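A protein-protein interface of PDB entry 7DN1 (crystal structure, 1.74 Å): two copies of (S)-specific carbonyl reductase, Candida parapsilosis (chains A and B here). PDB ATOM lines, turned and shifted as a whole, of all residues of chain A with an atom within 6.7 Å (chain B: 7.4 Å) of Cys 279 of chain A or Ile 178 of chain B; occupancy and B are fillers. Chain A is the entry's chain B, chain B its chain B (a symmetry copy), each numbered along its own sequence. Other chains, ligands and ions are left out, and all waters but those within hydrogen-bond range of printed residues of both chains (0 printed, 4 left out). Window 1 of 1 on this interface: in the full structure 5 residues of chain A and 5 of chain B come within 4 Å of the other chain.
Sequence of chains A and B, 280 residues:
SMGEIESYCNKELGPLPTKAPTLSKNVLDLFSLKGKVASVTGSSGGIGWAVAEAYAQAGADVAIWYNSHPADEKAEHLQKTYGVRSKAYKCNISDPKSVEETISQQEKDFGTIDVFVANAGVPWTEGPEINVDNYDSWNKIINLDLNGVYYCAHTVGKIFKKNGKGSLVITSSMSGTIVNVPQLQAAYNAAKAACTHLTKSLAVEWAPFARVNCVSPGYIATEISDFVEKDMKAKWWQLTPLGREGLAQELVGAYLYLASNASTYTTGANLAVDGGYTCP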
ATOM      1  N   ILE A 178      29.240  29.003 -27.405  1.00  0.00           N
ATOM      2  CA  ILE A 178      27.884  29.137 -27.925  1.00  0.00           C
ATOM      3  C   ILE A 178      27.941  29.504 -29.406  1.00  0.00           C
ATOM      4  O   ILE A 178      28.995  29.833 -29.949  1.00  0.00           O
ATOM      5  CB  ILE A 178      27.077  30.223 -27.225  1.00  0.00           C
ATOM      6  CG1 ILE A 178      27.827  31.516 -27.527  1.00  0.00           C
ATOM      7  CG2 ILE A 178      26.874  29.868 -25.740  1.00  0.00           C
ATOM      8  CD1 ILE A 178      27.125  32.583 -27.285  1.00  0.00           C
ATOM      9  N   PRO A 241      22.396  39.072 -20.083  1.00  0.00           N
ATOM     10  CA  PRO A 241      21.812  39.325 -18.750  1.00  0.00           C
ATOM     11  C   PRO A 241      22.132  40.685 -18.158  1.00  0.00           C
ATOM     12  O   PRO A 241      21.254  41.273 -17.508  1.00  0.00           O
ATOM     13  CB  PRO A 241      22.385  38.172 -17.916  1.00  0.00           C
ATOM     14  CG  PRO A 241      22.546  37.096 -18.924  1.00  0.00           C
ATOM     15  CD  PRO A 241      22.925  37.707 -20.210  1.00  0.00           C
ATOM     16  N   ASP A 274      31.363  38.002 -20.200  1.00  0.00           N
ATOM     17  CA  ASP A 274      30.427  38.153 -21.310  1.00  0.00           C
ATOM     18  C   ASP A 274      29.103  38.738 -20.837  1.00  0.00           C
ATOM     19  O   ASP A 274      28.094  38.592 -21.539  1.00  0.00           O
ATOM     20  CB  ASP A 274      30.080  36.803 -21.986  1.00  0.00           C
ATOM     21  CG  ASP A 274      29.624  35.729 -20.992  1.00  0.00           C
ATOM     22  OD1 ASP A 274      29.354  36.036 -19.809  1.00  0.00           O
ATOM     23  OD2 ASP A 274      29.509  34.556 -21.407  1.00  0.00           O
ATOM     24  N   GLY A 276      27.158  37.607 -18.683  1.00  0.00           N
ATOM     25  CA  GLY A 276      26.222  36.520 -18.498  1.00  0.00           C
ATOM     26  C   GLY A 276      25.715  35.859 -19.762  1.00  0.00           C
ATOM     27  O   GLY A 276      24.857  34.977 -19.669  1.00  0.00           O
ATOM     28  N   TYR A 277      26.240  36.222 -20.936  1.00  0.00           N
ATOM     29  CA  TYR A 277      25.581  35.827 -22.179  1.00  0.00           C
ATOM     30  C   TYR A 277      25.472  34.310 -22.322  1.00  0.00           C
ATOM     31  O   TYR A 277      24.484  33.813 -22.879  1.00  0.00           O
ATOM     32  CB  TYR A 277      26.315  36.378 -23.386  1.00  0.00           C
ATOM     33  CG  TYR A 277      25.511  36.183 -24.664  1.00  0.00           C
ATOM     34  CD1 TYR A 277      25.498  34.954 -25.325  1.00  0.00           C
ATOM     35  CD2 TYR A 277      24.810  37.218 -25.238  1.00  0.00           C
ATOM     36  CE1 TYR A 277      24.839  34.757 -26.499  1.00  0.00           C
ATOM     37  CE2 TYR A 277      24.108  37.004 -26.432  1.00  0.00           C
ATOM     38  CZ  TYR A 277      24.149  35.765 -27.046  1.00  0.00           C
ATOM     39  OH  TYR A 277      23.470  35.513 -28.223  1.00  0.00           O
ATOM     40  N   THR A 278      26.488  33.562 -21.884  1.00  0.00           N
ATOM     41  CA  THR A 278      26.449  32.105 -22.028  1.00  0.00           C
ATOM     42  C   THR A 278      25.508  31.420 -21.038  1.00  0.00           C
ATOM     43  O   THR A 278      25.397  30.187 -21.077  1.00  0.00           O
ATOM     44  CB  THR A 278      27.853  31.505 -21.881  1.00  0.00           C
ATOM     45  OG1 THR A 278      28.421  31.900 -20.628  1.00  0.00           O
ATOM     46  CG2 THR A 278      28.747  31.969 -23.029  1.00  0.00           C
ATOM     47  N   CYS A 279      24.825  32.167 -20.165  1.00  0.00           N
ATOM     48  CA  CYS A 279      23.979  31.555 -19.141  1.00  0.00           C
ATOM     49  C   CYS A 279      22.575  31.207 -19.649  1.00  0.00           C
ATOM     50  O   CYS A 279      22.118  30.075 -19.427  1.00  0.00           O
ATOM     51  CB  CYS A 279      23.908  32.470 -17.920  1.00  0.00           C
ATOM     52  SG  CYS A 279      25.460  32.482 -17.016  1.00  0.00           S
ATOM     53  N   PRO A 280      21.845  32.129 -20.322  1.00  0.00           N
ATOM     54  CA  PRO A 280      20.541  31.750 -20.894  1.00  0.00           C
ATOM     55  C   PRO A 280      20.635  30.695 -21.996  1.00  0.00           C
ATOM     56  O   PRO A 280      21.708  30.454 -22.565  1.00  0.00           O
ATOM     57  CB  PRO A 280      20.013  33.069 -21.480  1.00  0.00           C
ATOM     58  CG  PRO A 280      20.779  34.142 -20.767  1.00  0.00           C
ATOM     59  CD  PRO A 280      22.141  33.549 -20.574  1.00  0.00           C
ATOM     60  N   SER B 173      16.604  18.259 -17.638  1.00  0.00           N
ATOM     61  CA  SER B 173      15.971  19.313 -18.397  1.00  0.00           C
ATOM     62  C   SER B 173      17.088  20.144 -18.977  1.00  0.00           C
ATOM     63  O   SER B 173      18.212  20.148 -18.456  1.00  0.00           O
ATOM     64  CB  SER B 173      15.057  20.205 -17.539  1.00  0.00           C
ATOM     65  OG  SER B 173      14.710  21.365 -18.289  1.00  0.00           O
ATOM     66  N   MET B 174      16.765  20.881 -20.026  1.00  0.00           N
ATOM     67  CA  MET B 174      17.739  21.821 -20.544  1.00  0.00           C
ATOM     68  C   MET B 174      18.057  22.832 -19.452  1.00  0.00           C
ATOM     69  O   MET B 174      19.142  23.428 -19.418  1.00  0.00           O
ATOM     70  CB  MET B 174      17.151  22.483 -21.772  1.00  0.00           C
ATOM     71  CG  MET B 174      15.998  23.373 -21.537  1.00  0.00           C
ATOM     72  SD  MET B 174      15.782  23.807 -23.260  1.00  0.00           S
ATOM     73  CE  MET B 174      17.254  24.644 -23.456  1.00  0.00           C
ATOM     74  N   SER B 175      17.123  22.980 -18.504  1.00  0.00           N
ATOM     75  CA  SER B 175      17.268  23.894 -17.387  1.00  0.00           C
ATOM     76  C   SER B 175      18.409  23.516 -16.455  1.00  0.00           C
ATOM     77  O   SER B 175      18.793  24.333 -15.602  1.00  0.00           O
ATOM     78  CB  SER B 175      15.979  23.929 -16.563  1.00  0.00           C
ATOM     79  OG  SER B 175      14.858  24.368 -17.332  1.00  0.00           O
ATOM     80  N   GLY B 176      18.926  22.282 -16.533  1.00  0.00           N
ATOM     81  CA  GLY B 176      20.115  21.957 -15.759  1.00  0.00           C
ATOM     82  C   GLY B 176      21.414  22.438 -16.371  1.00  0.00           C
ATOM     83  O   GLY B 176      22.463  22.400 -15.705  1.00  0.00           O
ATOM     84  N   THR B 177      21.359  22.882 -17.636  1.00  0.00           N
ATOM     85  CA  THR B 177      22.527  23.363 -18.368  1.00  0.00           C
ATOM     86  C   THR B 177      22.458  24.839 -18.720  1.00  0.00           C
ATOM     87  O   THR B 177      23.504  25.498 -18.757  1.00  0.00           O
ATOM     88  CB  THR B 177      22.734  22.560 -19.668  1.00  0.00           C
ATOM     89  OG1 THR B 177      21.578  22.653 -20.490  1.00  0.00           O
ATOM     90  CG2 THR B 177      23.002  21.078 -19.373  1.00  0.00           C
ATOM     91  N   ILE B 178      21.258  25.380 -18.950  1.00  0.00           N
ATOM     92  CA  ILE B 178      21.058  26.797 -19.235  1.00  0.00           C
ATOM     93  C   ILE B 178      20.049  27.377 -18.247  1.00  0.00           C
ATOM     94  O   ILE B 178      19.389  26.655 -17.500  1.00  0.00           O
ATOM     95  CB  ILE B 178      20.513  27.055 -20.635  1.00  0.00           C
ATOM     96  CG1 ILE B 178      19.149  26.374 -20.651  1.00  0.00           C
ATOM     97  CG2 ILE B 178      21.530  26.601 -21.698  1.00  0.00           C
ATOM     98  CD1 ILE B 178      18.400  26.752 -21.643  1.00  0.00           C
ATOM     99  N   VAL B 179      19.883  28.702 -18.303  1.00  0.00           N
ATOM    100  CA  VAL B 179      18.937  29.416 -17.450  1.00  0.00           C
ATOM    101  C   VAL B 179      17.759  29.864 -18.313  1.00  0.00           C
ATOM    102  O   VAL B 179      17.924  30.704 -19.206  1.00  0.00           O
ATOM    103  CB  VAL B 179      19.593  30.623 -16.762  1.00  0.00           C
ATOM    104  CG1 VAL B 179      18.584  31.323 -15.853  1.00  0.00           C
ATOM    105  CG2 VAL B 179      20.849  30.184 -15.992  1.00  0.00           C
ATOM    106  N   ASN B 180      16.568  29.320 -18.050  1.00  0.00           N
ATOM    107  CA  ASN B 180      15.403  29.683 -18.852  1.00  0.00           C
ATOM    108  C   ASN B 180      15.096  31.166 -18.735  1.00  0.00           C
ATOM    109  O   ASN B 180      15.259  31.765 -17.667  1.00  0.00           O
ATOM    110  CB  ASN B 180      14.175  28.892 -18.423  1.00  0.00           C
ATOM    111  CG  ASN B 180      14.392  27.415 -18.530  1.00  0.00           C
ATOM    112  OD1 ASN B 180      15.194  26.842 -17.785  1.00  0.00           O
ATOM    113  ND2 ASN B 180      13.701  26.782 -19.484  1.00  0.00           N
ATOM    114  N   VAL B 181      14.657  31.738 -19.856  1.00  0.00           N
ATOM    115  CA  VAL B 181      14.130  33.104 -19.917  1.00  0.00           C
ATOM    116  C   VAL B 181      12.941  33.123 -20.854  1.00  0.00           C
ATOM    117  O   VAL B 181      12.833  32.300 -21.776  1.00  0.00           O
ATOM    118  CB  VAL B 181      15.195  34.108 -20.420  1.00  0.00           C
ATOM    119  CG1 VAL B 181      16.314  34.266 -19.413  1.00  0.00           C
ATOM    120  CG2 VAL B 181      15.717  33.706 -21.800  1.00  0.00           C
ATOM    121  N   GLN B 185      13.245  30.848 -12.905  1.00  0.00           N
ATOM    122  CA  GLN B 185      12.926  29.645 -12.125  1.00  0.00           C
ATOM    123  C   GLN B 185      14.187  29.018 -11.525  1.00  0.00           C
ATOM    124  O   GLN B 185      14.475  27.828 -11.700  1.00  0.00           O
ATOM    125  CB  GLN B 185      12.180  28.647 -13.010  1.00  0.00           C
ATOM    126  CG  GLN B 185      12.817  28.481 -14.395  1.00  0.00           C
ATOM    127  CD  GLN B 185      12.101  27.443 -15.243  1.00  0.00           C
ATOM    128  OE1 GLN B 185      10.876  27.511 -15.429  1.00  0.00           O
ATOM    129  NE2 GLN B 185      12.857  26.493 -15.777  1.00  0.00           N
ATOM    130  N   ASN B 189      15.951  25.172 -11.939  1.00  0.00           N
ATOM    131  CA  ASN B 189      17.207  25.005 -12.666  1.00  0.00           C
ATOM    132  C   ASN B 189      18.262  24.356 -11.781  1.00  0.00           C
ATOM    133  O   ASN B 189      19.019  23.478 -12.226  1.00  0.00           O
ATOM    134  CB  ASN B 189      17.729  26.350 -13.176  1.00  0.00           C
ATOM    135  CG  ASN B 189      16.720  27.119 -14.007  1.00  0.00           C
ATOM    136  OD1 ASN B 189      15.714  26.576 -14.501  1.00  0.00           O
ATOM    137  ND2 ASN B 189      16.978  28.420 -14.154  1.00  0.00           N
ATOM    138  N   ALA B 190      18.335  24.790 -10.521  1.00  0.00           N
ATOM    139  CA  ALA B 190      19.307  24.220  -9.596  1.00  0.00           C
ATOM    140  C   ALA B 190      19.046  22.737  -9.368  1.00  0.00           C
ATOM    141  O   ALA B 190      19.982  21.927  -9.355  1.00  0.00           O
ATOM    142  CB  ALA B 190      19.268  24.985  -8.273  1.00  0.00           C
ATOM    143  N   TYR B 219      11.791  22.465 -24.609  1.00  0.00           N
ATOM    144  CA  TYR B 219      10.375  22.758 -24.443  1.00  0.00           C
ATOM    145  C   TYR B 219       9.552  21.702 -25.173  1.00  0.00           C
ATOM    146  O   TYR B 219       9.590  21.628 -26.406  1.00  0.00           O
ATOM    147  CB  TYR B 219      10.056  24.153 -24.977  1.00  0.00           C
ATOM    148  CG  TYR B 219      10.637  25.224 -24.085  1.00  0.00           C
ATOM    149  CD1 TYR B 219      10.121  25.446 -22.816  1.00  0.00           C
ATOM    150  CD2 TYR B 219      11.723  25.981 -24.498  1.00  0.00           C
ATOM    151  CE1 TYR B 219      10.683  26.405 -21.966  1.00  0.00           C
ATOM    152  CE2 TYR B 219      12.279  26.948 -23.666  1.00  0.00           C
ATOM    153  CZ  TYR B 219      11.759  27.147 -22.401  1.00  0.00           C
ATOM    154  OH  TYR B 219      12.308  28.113 -21.579  1.00  0.00           O
ATOM    155  N   ASP B 274      16.383  19.122 -27.578  1.00  0.00           N
ATOM    156  CA  ASP B 274      15.849  20.434 -27.230  1.00  0.00           C
ATOM    157  C   ASP B 274      15.701  21.315 -28.464  1.00  0.00           C
ATOM    158  O   ASP B 274      15.625  22.542 -28.324  1.00  0.00           O
ATOM    159  CB  ASP B 274      16.768  21.215 -26.257  1.00  0.00           C
ATOM    160  CG  ASP B 274      18.223  21.294 -26.734  1.00  0.00           C
ATOM    161  OD1 ASP B 274      18.526  20.955 -27.900  1.00  0.00           O
ATOM    162  OD2 ASP B 274      19.080  21.729 -25.936  1.00  0.00           O
ATOM    163  N   TYR B 277      18.202  24.191 -28.552  1.00  0.00           N
ATOM    164  CA  TYR B 277      18.057  25.388 -27.726  1.00  0.00           C
ATOM    165  C   TYR B 277      19.340  25.734 -26.974  1.00  0.00           C
ATOM    166  O   TYR B 277      19.637  26.920 -26.775  1.00  0.00           O
ATOM    167  CB  TYR B 277      16.933  25.223 -26.720  1.00  0.00           C
ATOM    168  CG  TYR B 277      16.612  26.539 -26.024  1.00  0.00           C
ATOM    169  CD1 TYR B 277      17.394  27.003 -24.965  1.00  0.00           C
ATOM    170  CD2 TYR B 277      15.518  27.292 -26.379  1.00  0.00           C
ATOM    171  CE1 TYR B 277      17.106  28.143 -24.281  1.00  0.00           C
ATOM    172  CE2 TYR B 277      15.240  28.482 -25.692  1.00  0.00           C
ATOM    173  CZ  TYR B 277      16.046  28.877 -24.640  1.00  0.00           C
ATOM    174  OH  TYR B 277      15.807  30.044 -23.938  1.00  0.00           O
ATOM    175  N   THR B 278      20.084  24.730 -26.502  1.00  0.00           N
ATOM    176  CA  THR B 278      21.307  25.009 -25.746  1.00  0.00           C
ATOM    177  C   THR B 278      22.472  25.470 -26.620  1.00  0.00           C
ATOM    178  O   THR B 278      23.554  25.737 -26.079  1.00  0.00           O
ATOM    179  CB  THR B 278      21.742  23.778 -24.941  1.00  0.00           C
ATOM    180  OG1 THR B 278      21.902  22.657 -25.817  1.00  0.00           O
ATOM    181  CG2 THR B 278      20.705  23.456 -23.867  1.00  0.00           C
ATOM    182  N   CYS B 279      22.292  25.583 -27.939  1.00  0.00           N
ATOM    183  CA  CYS B 279      23.398  25.937 -28.829  1.00  0.00           C
ATOM    184  C   CYS B 279      23.633  27.448 -28.926  1.00  0.00           C
ATOM    185  O   CYS B 279      24.785  27.889 -28.788  1.00  0.00           O
ATOM    186  CB  CYS B 279      23.159  25.331 -30.210  1.00  0.00           C
ATOM    187  SG  CYS B 279      23.384  23.548 -30.195  1.00  0.00           S
ATOM    188  N   PRO B 280      22.596  28.286 -29.167  1.00  0.00           N
ATOM    189  CA  PRO B 280      22.817  29.743 -29.155  1.00  0.00           C
ATOM    190  C   PRO B 280      23.231  30.292 -27.791  1.00  0.00           C
ATOM    191  O   PRO B 280      23.060  29.634 -26.755  1.00  0.00           O
ATOM    192  CB  PRO B 280      21.446  30.314 -29.552  1.00  0.00           C
ATOM    193  CG  PRO B 280      20.740  29.182 -30.234  1.00  0.00           C
ATOM    194  CD  PRO B 280      21.195  27.967 -29.487  1.00  0.00           C
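The backbone carbonyl oxygen (O) of Cys 279 of chain A is in hydrogen-bond range of the backbone NH (N) of Val 179 of chain B (2.9 Å).
O of Gly 276 of chain A sits close to SG of Cys 279 of chain A (3.7 Å).
Among the printed residues, pairs that only touch across the chains: Pro 280 of chain A with Val 179 of chain B (3.3 Å), Cys 279 of chain A with Ile 178 of chain B (3.5 Å), Ile 178 of chain A with Cys 279 of chain B (3.5 Å), Pro 280 of chain A with Ile 178 of chain B (3.9 Å) and Ile 178 of chain A with Pro 280 of chain B (3.9 Å).
Of the printed residues of chain B, Ile 178 of chain A touches Cys 279 and Pro 280.
Of the printed residues of chain B, Pro 280 of chain A touches Ile 178 (3.9 Å) and Val 179 (3.3 Å).
Met 174 of chain B touches none of the printed residues of chain A.
Of chain A, only Cys 279 and Pro 280 come within 4 Å of Ile 178 of chain B.
Printed residues of chain A within 4 Å of Val 179 of chain B: Cys 279 (2.9 Å) and Pro 280 (3.3 Å).
Printed residues of chain A within 4 Å of Cys 279 of chain B: Ile 178.
Printed residues of chain A within 4 Å of Pro 280 of chain B: Ile 178 (3.9 Å).
The nearest residue of chain B that does not touch Cys 279 of chain A is Thr 177 of chain B (4.8 Å).
The nearest residue of chain A that does not touch Ile 178 of chain B is Thr 278 of chain A (5.3 Å).
The nearest printed residue of chain A that does not touch Pro 280 of chain B is Pro 280 of chain A (4.5 Å).
Of the 18 printed residues of chain B, 4 touch a printed residue of chain A.
Of the 8 printed residues of chain A, 3 touch a printed residue of chain B.
Printed residues of chain A that touch a printed residue of chain B: Ile 178, Cys 279 and Pro 280.
Hydrophobic or aromatic side chains of chain A that line the printed part of chain B: Ile 178 and Pro 280.
Among the printed residues, no Asp or Glu carboxylate lies within 4 Å of a Lys or Arg side-chain nitrogen of the other chain.
Ile 178 of chain A touches Cys 279 of chain B, and with the chains exchanged Cys 279 of chain A touches Ile 178 of chain B.
Ile 178 of chain A touches Pro 280 of chain B, and with the chains exchanged Pro 280 of chain A touches Ile 178 of chain B.
Of the 6 pairs that touch across the chains among the printed residues, 4 have their exchanged pair printed and touching as well.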
